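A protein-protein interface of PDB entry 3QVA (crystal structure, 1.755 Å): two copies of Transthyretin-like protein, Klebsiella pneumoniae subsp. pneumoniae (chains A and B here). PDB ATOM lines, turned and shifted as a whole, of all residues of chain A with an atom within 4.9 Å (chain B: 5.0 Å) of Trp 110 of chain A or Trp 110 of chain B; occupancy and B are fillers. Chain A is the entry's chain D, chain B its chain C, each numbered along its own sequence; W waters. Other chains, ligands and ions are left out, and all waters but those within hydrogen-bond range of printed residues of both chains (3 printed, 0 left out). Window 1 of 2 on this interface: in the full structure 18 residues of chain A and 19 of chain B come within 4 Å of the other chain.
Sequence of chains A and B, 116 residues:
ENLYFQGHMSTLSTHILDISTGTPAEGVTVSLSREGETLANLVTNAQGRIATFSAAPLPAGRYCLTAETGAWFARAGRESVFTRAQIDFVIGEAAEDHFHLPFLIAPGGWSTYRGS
The backbone carbonyl oxygen of Trp 110 of chain A sits at hydrogen-bond distance from the backbone NH of Thr 112 of chain B (2.9 Å).
The backbone carbonyl oxygen of Trp 110 of chain B is in hydrogen-bond range of the backbone NH of Thr 112 of chain A, 2.9 Å away.
The side-chain amide oxygen (OE1) of Gln 86 of chain B is in hydrogen-bond range of the side-chain amide nitrogen (NE2) of Gln 86 of chain A, 3.2 Å away.
N of Leu 104 of chain B is in hydrogen-bond range of O of Ser 111 of chain B (2.9 Å).
The guanidinium group (NH2) of Arg 84 of chain A lies close to the side-chain amide nitrogen (NE2) of Gln 86 of chain A (3.1 Å).
N of Leu 104 of chain A sits at hydrogen-bond distance from O of Ser 111 of chain A (2.9 Å).
Among the printed residues, merely in contact across the chains: Ser 111 of chain A with Ser 111 of chain B (3.2 Å), Gly 109 of chain A with Thr 112 of chain B (3.3 Å), Thr 112 of chain A with Gly 109 of chain B (3.3 Å), Trp 110 of chain A with Ser 111 of chain B (3.4 Å), Ile 87 of chain A with Phe 82 of chain B (3.4 Å), Ser 111 of chain A with Trp 110 of chain B (3.4 Å), Arg 84 of chain A with Gln 86 of chain B (3.5 Å), Phe 82 of chain A with Ile 87 of chain B (3.6 Å), Trp 110 of chain A with Trp 110 of chain B (3.6 Å), Thr 112 of chain A with Phe 82 of chain B (3.8 Å), Phe 82 of chain A with Thr 112 of chain B (3.8 Å) and Trp 110 of chain A with Gln 86 of chain B (3.96 Å).
Trp 110 of chain A touches just these residues of chain B: Gln 86, Trp 110, Ser 111 and Thr 112.
Trp 110 of chain B touches just these residues of chain A: Trp 110 (3.6 Å), Ser 111 (3.4 Å) and Thr 112 (2.9 Å).
Of the printed residues of chain A, Thr 112 of chain B touches Phe 82 (3.8 Å), Gly 109 (3.3 Å) and Trp 110 (2.9 Å).
Of the printed residues of chain A, Phe 82 of chain B touches Ile 87 and Thr 112.
Printed residues of chain B within 4 Å of Gly 109 of chain A: Thr 112 (3.3 Å).
Of the printed residues of chain B, Arg 84 of chain A touches Gln 86 (3.5 Å).
Of the printed residues of chain B, Gln 86 of chain A touches Gln 86 (3.2 Å).
The nearest printed residue of chain B that does not touch Ser 111 of chain A is Thr 112 of chain B (5.1 Å).
Printed residues of chain A that touch a printed residue of chain B: Phe 82, Arg 84, Gln 86, Ile 87, Gly 109, Trp 110, Ser 111 and Thr 112.
Of the 14 printed residues of chain B, 7 touch a printed residue of chain A.
Hydrophobic or aromatic side chains of chain B that line the printed part of chain A: Phe 82, Ile 87 and Trp 110.
Among the printed residues, 15 pairs touch across the chains.
Phe 82 of chain A touches Thr 112 of chain B, and with the chains exchanged Thr 112 of chain A touches Phe 82 of chain B.
Gln 86 of chain B touches its own counterpart, Gln 86 of chain A.
Trp 110 of chain A touches Ser 111 of chain B, and with the chains exchanged Ser 111 of chain A touches Trp 110 of chain B.
Trp 110 of chain A touches Thr 112 of chain B, and with the chains exchanged Thr 112 of chain A touches Trp 110 of chain B.
Water W3 bridges O of Gln 86 of chain B (2.7 Å) and N of Gln 86 of chain A (3.0 Å).
Water W2 bridges the backbone carbonyl oxygen (O) of Gln 86 of chain A (2.7 Å) and the backbone NH (N) of Gln 86 of chain B (2.9 Å).
Water W1 bridges the side-chain amide oxygen (OE1) of Gln 86 of chain B (3.2 Å) and the side-chain amide nitrogen (NE2) of Gln 86 of chain A (3.2 Å).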
ATOM      1  N   PHE A  82      -9.606 -11.794 -12.572  1.00  0.00           N
ATOM      2  CA  PHE A  82      -9.686 -10.563 -13.369  1.00  0.00           C
ATOM      3  C   PHE A  82      -9.973  -9.374 -12.473  1.00  0.00           C
ATOM      4  O   PHE A  82     -10.942  -9.378 -11.716  1.00  0.00           O
ATOM      5  CB  PHE A  82     -10.722 -10.690 -14.491  1.00  0.00           C
ATOM      6  CG  PHE A  82     -10.453 -11.843 -15.425  1.00  0.00           C
ATOM      7  CD1 PHE A  82     -11.171 -13.027 -15.308  1.00  0.00           C
ATOM      8  CD2 PHE A  82      -9.459 -11.756 -16.394  1.00  0.00           C
ATOM      9  CE1 PHE A  82     -10.911 -14.110 -16.150  1.00  0.00           C
ATOM     10  CE2 PHE A  82      -9.194 -12.841 -17.248  1.00  0.00           C
ATOM     11  CZ  PHE A  82      -9.931 -14.015 -17.123  1.00  0.00           C
ATOM     12  N   ARG A  84     -10.349  -6.069 -13.428  1.00  0.00           N
ATOM     13  CA  ARG A  84     -11.205  -5.067 -14.054  1.00  0.00           C
ATOM     14  C   ARG A  84     -11.404  -5.508 -15.501  1.00  0.00           C
ATOM     15  O   ARG A  84     -10.745  -6.443 -15.962  1.00  0.00           O
ATOM     16  CB  ARG A  84     -10.531  -3.691 -14.021  1.00  0.00           C
ATOM     17  CG  ARG A  84      -9.240  -3.654 -14.818  1.00  0.00           C
ATOM     18  CD  ARG A  84      -8.194  -2.738 -14.219  1.00  0.00           C
ATOM     19  NE  ARG A  84      -8.384  -1.336 -14.577  1.00  0.00           N
ATOM     20  CZ  ARG A  84      -8.003  -0.789 -15.730  1.00  0.00           C
ATOM     21  NH1 ARG A  84      -8.218   0.503 -15.948  1.00  0.00           N
ATOM     22  NH2 ARG A  84      -7.423  -1.526 -16.674  1.00  0.00           N
ATOM     23  N   ALA A  85     -12.297  -4.828 -16.209  1.00  0.00           N
ATOM     24  CA  ALA A  85     -12.553  -5.115 -17.615  1.00  0.00           C
ATOM     25  C   ALA A  85     -12.478  -3.815 -18.416  1.00  0.00           C
ATOM     26  O   ALA A  85     -13.338  -2.945 -18.294  1.00  0.00           O
ATOM     27  CB  ALA A  85     -13.913  -5.777 -17.777  1.00  0.00           C
ATOM     28  N   GLN A  86     -11.433  -3.699 -19.228  1.00  0.00           N
ATOM     29  CA  GLN A  86     -11.200  -2.512 -20.044  1.00  0.00           C
ATOM     30  C   GLN A  86     -11.449  -2.841 -21.505  1.00  0.00           C
ATOM     31  O   GLN A  86     -10.889  -3.803 -22.035  1.00  0.00           O
ATOM     32  CB  GLN A  86      -9.762  -2.003 -19.869  1.00  0.00           C
ATOM     33  CG  GLN A  86      -9.416  -0.787 -20.717  1.00  0.00           C
ATOM     34  CD  GLN A  86      -7.962  -0.344 -20.583  1.00  0.00           C
ATOM     35  OE1 GLN A  86      -7.215  -0.348 -21.559  1.00  0.00           O
ATOM     36  NE2 GLN A  86      -7.558   0.040 -19.373  1.00  0.00           N
ATOM     37  N   ILE A  87     -12.293  -2.032 -22.139  1.00  0.00           N
ATOM     38  CA  ILE A  87     -12.530  -2.105 -23.575  1.00  0.00           C
ATOM     39  C   ILE A  87     -11.813  -0.921 -24.216  1.00  0.00           C
ATOM     40  O   ILE A  87     -11.912   0.208 -23.738  1.00  0.00           O
ATOM     41  CB  ILE A  87     -14.044  -2.025 -23.900  1.00  0.00           C
ATOM     42  CG1 ILE A  87     -14.790  -3.230 -23.329  1.00  0.00           C
ATOM     43  CG2 ILE A  87     -14.283  -1.916 -25.420  1.00  0.00           C
ATOM     44  CD1 ILE A  87     -16.323  -3.068 -23.395  1.00  0.00           C
ATOM     45  N   PHE A 103     -20.833  -5.572 -21.387  1.00  0.00           N
ATOM     46  CA  PHE A 103     -19.871  -6.470 -20.767  1.00  0.00           C
ATOM     47  C   PHE A 103     -20.651  -7.673 -20.258  1.00  0.00           C
ATOM     48  O   PHE A 103     -21.637  -7.511 -19.533  1.00  0.00           O
ATOM     49  CB  PHE A 103     -19.216  -5.845 -19.533  1.00  0.00           C
ATOM     50  CG  PHE A 103     -18.362  -4.628 -19.799  1.00  0.00           C
ATOM     51  CD1 PHE A 103     -16.969  -4.720 -19.761  1.00  0.00           C
ATOM     52  CD2 PHE A 103     -18.944  -3.383 -19.978  1.00  0.00           C
ATOM     53  CE1 PHE A 103     -16.171  -3.594 -19.945  1.00  0.00           C
ATOM     54  CE2 PHE A 103     -18.162  -2.246 -20.182  1.00  0.00           C
ATOM     55  CZ  PHE A 103     -16.764  -2.354 -20.158  1.00  0.00           C
ATOM     56  N   LEU A 104     -20.209  -8.871 -20.619  1.00  0.00           N
ATOM     57  CA  LEU A 104     -20.775 -10.091 -20.067  1.00  0.00           C
ATOM     58  C   LEU A 104     -19.733 -10.603 -19.098  1.00  0.00           C
ATOM     59  O   LEU A 104     -18.616 -10.933 -19.497  1.00  0.00           O
ATOM     60  CB  LEU A 104     -21.065 -11.112 -21.174  1.00  0.00           C
ATOM     61  CG  LEU A 104     -21.955 -10.613 -22.319  1.00  0.00           C
ATOM     62  CD1 LEU A 104     -22.278 -11.781 -23.230  1.00  0.00           C
ATOM     63  CD2 LEU A 104     -23.243  -9.964 -21.806  1.00  0.00           C
ATOM     64  N   ILE A 105     -20.066 -10.624 -17.814  1.00  0.00           N
ATOM     65  CA  ILE A 105     -19.037 -10.866 -16.802  1.00  0.00           C
ATOM     66  C   ILE A 105     -19.286 -12.082 -15.913  1.00  0.00           C
ATOM     67  O   ILE A 105     -20.425 -12.472 -15.678  1.00  0.00           O
ATOM     68  CB  ILE A 105     -18.777  -9.606 -15.924  1.00  0.00           C
ATOM     69  CG1 ILE A 105     -19.967  -9.311 -14.994  1.00  0.00           C
ATOM     70  CG2 ILE A 105     -18.431  -8.394 -16.802  1.00  0.00           C
ATOM     71  CD1 ILE A 105     -19.681  -8.200 -14.001  1.00  0.00           C
ATOM     72  N   ALA A 106     -18.191 -12.660 -15.429  1.00  0.00           N
ATOM     73  CA  ALA A 106     -18.228 -13.769 -14.476  1.00  0.00           C
ATOM     74  C   ALA A 106     -16.882 -13.791 -13.759  1.00  0.00           C
ATOM     75  O   ALA A 106     -15.890 -13.259 -14.279  1.00  0.00           O
ATOM     76  CB  ALA A 106     -18.471 -15.099 -15.205  1.00  0.00           C
ATOM     77  N   GLY A 108     -14.767 -16.041 -13.646  1.00  0.00           N
ATOM     78  CA  GLY A 108     -13.753 -16.754 -14.424  1.00  0.00           C
ATOM     79  C   GLY A 108     -13.653 -16.364 -15.889  1.00  0.00           C
ATOM     80  O   GLY A 108     -13.000 -17.058 -16.666  1.00  0.00           O
ATOM     81  N   GLY A 109     -14.261 -15.241 -16.263  1.00  0.00           N
ATOM     82  CA  GLY A 109     -14.176 -14.774 -17.639  1.00  0.00           C
ATOM     83  C   GLY A 109     -15.087 -13.613 -17.955  1.00  0.00           C
ATOM     84  O   GLY A 109     -16.056 -13.348 -17.240  1.00  0.00           O
ATOM     85  N   TRP A 110     -14.772 -12.905 -19.034  1.00  0.00           N
ATOM     86  CA  TRP A 110     -15.635 -11.829 -19.487  1.00  0.00           C
ATOM     87  C   TRP A 110     -15.532 -11.601 -20.994  1.00  0.00           C
ATOM     88  O   TRP A 110     -14.554 -12.022 -21.635  1.00  0.00           O
ATOM     89  CB  TRP A 110     -15.394 -10.536 -18.686  1.00  0.00           C
ATOM     90  CG  TRP A 110     -14.060  -9.866 -18.941  1.00  0.00           C
ATOM     91  CD1 TRP A 110     -12.871 -10.168 -18.365  1.00  0.00           C
ATOM     92  CD2 TRP A 110     -13.813  -8.768 -19.829  1.00  0.00           C
ATOM     93  NE1 TRP A 110     -11.881  -9.335 -18.840  1.00  0.00           N
ATOM     94  CE2 TRP A 110     -12.435  -8.461 -19.739  1.00  0.00           C
ATOM     95  CE3 TRP A 110     -14.623  -8.014 -20.688  1.00  0.00           C
ATOM     96  CZ2 TRP A 110     -11.842  -7.425 -20.478  1.00  0.00           C
ATOM     97  CZ3 TRP A 110     -14.030  -6.974 -21.429  1.00  0.00           C
ATOM     98  CH2 TRP A 110     -12.656  -6.701 -21.318  1.00  0.00           C
ATOM     99  N   SER A 111     -16.559 -10.952 -21.537  1.00  0.00           N
ATOM    100  CA  SER A 111     -16.701 -10.723 -22.970  1.00  0.00           C
ATOM    101  C   SER A 111     -17.238  -9.335 -23.206  1.00  0.00           C
ATOM    102  O   SER A 111     -17.921  -8.758 -22.353  1.00  0.00           O
ATOM    103  CB  SER A 111     -17.730 -11.680 -23.587  1.00  0.00           C
ATOM    104  OG  SER A 111     -17.603 -13.000 -23.110  1.00  0.00           O
ATOM    105  N   THR A 112     -16.958  -8.824 -24.396  1.00  0.00           N
ATOM    106  CA  THR A 112     -17.629  -7.651 -24.904  1.00  0.00           C
ATOM    107  C   THR A 112     -17.917  -7.835 -26.387  1.00  0.00           C
ATOM    108  O   THR A 112     -17.346  -8.705 -27.054  1.00  0.00           O
ATOM    109  CB  THR A 112     -16.802  -6.369 -24.680  1.00  0.00           C
ATOM    110  OG1 THR A 112     -17.561  -5.241 -25.125  1.00  0.00           O
ATOM    111  CG2 THR A 112     -15.473  -6.421 -25.444  1.00  0.00           C
ATOM    112  N   PHE B  82     -12.766  -2.483 -32.078  1.00  0.00           N
ATOM    113  CA  PHE B  82     -11.850  -2.714 -30.952  1.00  0.00           C
ATOM    114  C   PHE B  82     -10.400  -2.560 -31.385  1.00  0.00           C
ATOM    115  O   PHE B  82      -9.952  -3.203 -32.329  1.00  0.00           O
ATOM    116  CB  PHE B  82     -12.112  -4.079 -30.305  1.00  0.00           C
ATOM    117  CG  PHE B  82     -13.523  -4.234 -29.803  1.00  0.00           C
ATOM    118  CD1 PHE B  82     -14.469  -4.930 -30.552  1.00  0.00           C
ATOM    119  CD2 PHE B  82     -13.913  -3.646 -28.605  1.00  0.00           C
ATOM    120  CE1 PHE B  82     -15.786  -5.051 -30.105  1.00  0.00           C
ATOM    121  CE2 PHE B  82     -15.231  -3.763 -28.138  1.00  0.00           C
ATOM    122  CZ  PHE B  82     -16.169  -4.469 -28.894  1.00  0.00           C
ATOM    123  N   ARG B  84      -7.530  -2.959 -29.529  1.00  0.00           N
ATOM    124  CA  ARG B  84      -6.662  -3.957 -28.907  1.00  0.00           C
ATOM    125  C   ARG B  84      -7.487  -4.694 -27.861  1.00  0.00           C
ATOM    126  O   ARG B  84      -8.627  -4.321 -27.595  1.00  0.00           O
ATOM    127  CB  ARG B  84      -5.427  -3.309 -28.257  1.00  0.00           C
ATOM    128  CG  ARG B  84      -5.731  -2.244 -27.203  1.00  0.00           C
ATOM    129  CD  ARG B  84      -4.453  -1.506 -26.820  1.00  0.00           C
ATOM    130  NE  ARG B  84      -3.654  -1.218 -28.006  1.00  0.00           N
ATOM    131  CZ  ARG B  84      -3.896  -0.212 -28.840  1.00  0.00           C
ATOM    132  NH1 ARG B  84      -4.913   0.611 -28.608  1.00  0.00           N
ATOM    133  NH2 ARG B  84      -3.121  -0.027 -29.899  1.00  0.00           N
ATOM    134  N   ALA B  85      -6.916  -5.745 -27.281  1.00  0.00           N
ATOM    135  CA  ALA B  85      -7.595  -6.507 -26.253  1.00  0.00           C
ATOM    136  C   ALA B  85      -6.677  -6.599 -25.045  1.00  0.00           C
ATOM    137  O   ALA B  85      -5.608  -7.199 -25.120  1.00  0.00           O
ATOM    138  CB  ALA B  85      -7.954  -7.905 -26.779  1.00  0.00           C
ATOM    139  N   GLN B  86      -7.077  -5.968 -23.943  1.00  0.00           N
ATOM    140  CA  GLN B  86      -6.254  -5.928 -22.737  1.00  0.00           C
ATOM    141  C   GLN B  86      -6.930  -6.718 -21.624  1.00  0.00           C
ATOM    142  O   GLN B  86      -8.090  -6.462 -21.309  1.00  0.00           O
ATOM    143  CB  GLN B  86      -6.040  -4.473 -22.303  1.00  0.00           C
ATOM    144  CG  GLN B  86      -5.234  -4.310 -21.023  1.00  0.00           C
ATOM    145  CD  GLN B  86      -5.111  -2.859 -20.589  1.00  0.00           C
ATOM    146  OE1 GLN B  86      -5.637  -2.465 -19.546  1.00  0.00           O
ATOM    147  NE2 GLN B  86      -4.422  -2.055 -21.390  1.00  0.00           N
ATOM    148  N   ILE B  87      -6.201  -7.689 -21.066  1.00  0.00           N
ATOM    149  CA  ILE B  87      -6.657  -8.488 -19.930  1.00  0.00           C
ATOM    150  C   ILE B  87      -5.890  -8.022 -18.690  1.00  0.00           C
ATOM    151  O   ILE B  87      -4.658  -7.994 -18.687  1.00  0.00           O
ATOM    152  CB  ILE B  87      -6.387  -9.996 -20.147  1.00  0.00           C
ATOM    153  CG1 ILE B  87      -7.154 -10.523 -21.370  1.00  0.00           C
ATOM    154  CG2 ILE B  87      -6.765 -10.801 -18.890  1.00  0.00           C
ATOM    155  CD1 ILE B  87      -6.829 -11.981 -21.697  1.00  0.00           C
ATOM    156  N   PHE B 103      -7.595 -15.535 -25.768  1.00  0.00           N
ATOM    157  CA  PHE B 103      -8.379 -14.454 -26.362  1.00  0.00           C
ATOM    158  C   PHE B 103      -9.209 -15.077 -27.476  1.00  0.00           C
ATOM    159  O   PHE B 103      -8.652 -15.665 -28.406  1.00  0.00           O
ATOM    160  CB  PHE B 103      -7.485 -13.388 -27.006  1.00  0.00           C
ATOM    161  CG  PHE B 103      -6.627 -12.596 -26.042  1.00  0.00           C
ATOM    162  CD1 PHE B 103      -6.992 -11.315 -25.665  1.00  0.00           C
ATOM    163  CD2 PHE B 103      -5.417 -13.112 -25.579  1.00  0.00           C
ATOM    164  CE1 PHE B 103      -6.183 -10.559 -24.814  1.00  0.00           C
ATOM    165  CE2 PHE B 103      -4.606 -12.375 -24.724  1.00  0.00           C
ATOM    166  CZ  PHE B 103      -4.992 -11.092 -24.342  1.00  0.00           C
ATOM    167  N   LEU B 104     -10.526 -14.968 -27.386  1.00  0.00           N
ATOM    168  CA  LEU B 104     -11.383 -15.396 -28.492  1.00  0.00           C
ATOM    169  C   LEU B 104     -11.829 -14.122 -29.189  1.00  0.00           C
ATOM    170  O   LEU B 104     -12.563 -13.317 -28.620  1.00  0.00           O
ATOM    171  CB  LEU B 104     -12.566 -16.232 -27.990  1.00  0.00           C
ATOM    172  CG  LEU B 104     -12.196 -17.378 -27.036  1.00  0.00           C
ATOM    173  CD1 LEU B 104     -13.456 -18.035 -26.528  1.00  0.00           C
ATOM    174  CD2 LEU B 104     -11.270 -18.410 -27.681  1.00  0.00           C
ATOM    175  N   ILE B 105     -11.352 -13.916 -30.414  1.00  0.00           N
ATOM    176  CA  ILE B 105     -11.490 -12.606 -31.047  1.00  0.00           C
ATOM    177  C   ILE B 105     -12.295 -12.619 -32.343  1.00  0.00           C
ATOM    178  O   ILE B 105     -12.405 -13.654 -33.014  1.00  0.00           O
ATOM    179  CB  ILE B 105     -10.101 -11.942 -31.286  1.00  0.00           C
ATOM    180  CG1 ILE B 105      -9.359 -12.625 -32.442  1.00  0.00           C
ATOM    181  CG2 ILE B 105      -9.260 -11.969 -29.989  1.00  0.00           C
ATOM    182  CD1 ILE B 105      -8.008 -11.969 -32.813  1.00  0.00           C
ATOM    183  N   ALA B 106     -12.843 -11.447 -32.665  1.00  0.00           N
ATOM    184  CA  ALA B 106     -13.574 -11.183 -33.909  1.00  0.00           C
ATOM    185  C   ALA B 106     -13.633  -9.671 -34.101  1.00  0.00           C
ATOM    186  O   ALA B 106     -13.499  -8.916 -33.132  1.00  0.00           O
ATOM    187  CB  ALA B 106     -14.991 -11.757 -33.839  1.00  0.00           C
ATOM    188  N   GLY B 108     -16.082  -7.805 -34.358  1.00  0.00           N
ATOM    189  CA  GLY B 108     -17.176  -7.215 -33.599  1.00  0.00           C
ATOM    190  C   GLY B 108     -17.264  -7.604 -32.137  1.00  0.00           C
ATOM    191  O   GLY B 108     -18.258  -7.316 -31.485  1.00  0.00           O
ATOM    192  N   GLY B 109     -16.236  -8.258 -31.616  1.00  0.00           N
ATOM    193  CA  GLY B 109     -16.236  -8.608 -30.200  1.00  0.00           C
ATOM    194  C   GLY B 109     -15.119  -9.538 -29.802  1.00  0.00           C
ATOM    195  O   GLY B 109     -14.483 -10.172 -30.649  1.00  0.00           O
ATOM    196  N   TRP B 110     -14.865  -9.614 -28.501  1.00  0.00           N
ATOM    197  CA  TRP B 110     -13.857 -10.524 -28.017  1.00  0.00           C
ATOM    198  C   TRP B 110     -14.128 -10.945 -26.581  1.00  0.00           C
ATOM    199  O   TRP B 110     -14.915 -10.311 -25.868  1.00  0.00           O
ATOM    200  CB  TRP B 110     -12.450  -9.925 -28.180  1.00  0.00           C
ATOM    201  CG  TRP B 110     -12.138  -8.771 -27.267  1.00  0.00           C
ATOM    202  CD1 TRP B 110     -12.466  -7.454 -27.451  1.00  0.00           C
ATOM    203  CD2 TRP B 110     -11.415  -8.837 -26.034  1.00  0.00           C
ATOM    204  NE1 TRP B 110     -11.993  -6.696 -26.394  1.00  0.00           N
ATOM    205  CE2 TRP B 110     -11.340  -7.520 -25.517  1.00  0.00           C
ATOM    206  CE3 TRP B 110     -10.822  -9.883 -25.311  1.00  0.00           C
ATOM    207  CZ2 TRP B 110     -10.698  -7.222 -24.304  1.00  0.00           C
ATOM    208  CZ3 TRP B 110     -10.176  -9.587 -24.110  1.00  0.00           C
ATOM    209  CH2 TRP B 110     -10.123  -8.263 -23.617  1.00  0.00           C
ATOM    210  N   SER B 111     -13.510 -12.051 -26.185  1.00  0.00           N
ATOM    211  CA  SER B 111     -13.672 -12.548 -24.830  1.00  0.00           C
ATOM    212  C   SER B 111     -12.420 -13.230 -24.319  1.00  0.00           C
ATOM    213  O   SER B 111     -11.506 -13.556 -25.084  1.00  0.00           O
ATOM    214  CB  SER B 111     -14.876 -13.490 -24.734  1.00  0.00           C
ATOM    215  OG  SER B 111     -14.707 -14.635 -25.536  1.00  0.00           O
ATOM    216  N   THR B 112     -12.383 -13.409 -23.005  1.00  0.00           N
ATOM    217  CA  THR B 112     -11.326 -14.151 -22.350  1.00  0.00           C
ATOM    218  C   THR B 112     -11.915 -14.961 -21.209  1.00  0.00           C
ATOM    219  O   THR B 112     -13.041 -14.715 -20.764  1.00  0.00           O
ATOM    220  CB  THR B 112     -10.196 -13.229 -21.826  1.00  0.00           C
ATOM    221  OG1 THR B 112      -9.128 -14.043 -21.331  1.00  0.00           O
ATOM    222  CG2 THR B 112     -10.709 -12.289 -20.717  1.00  0.00           C
HETATM  223  O   HOH W   1      -4.550   0.163 -18.187  1.00  0.00           O
HETATM  224  O   HOH W   2      -9.105  -3.890 -24.071  1.00  0.00           O
HETATM  225  O   HOH W   3      -9.114  -5.526 -18.997  1.00  0.00           O
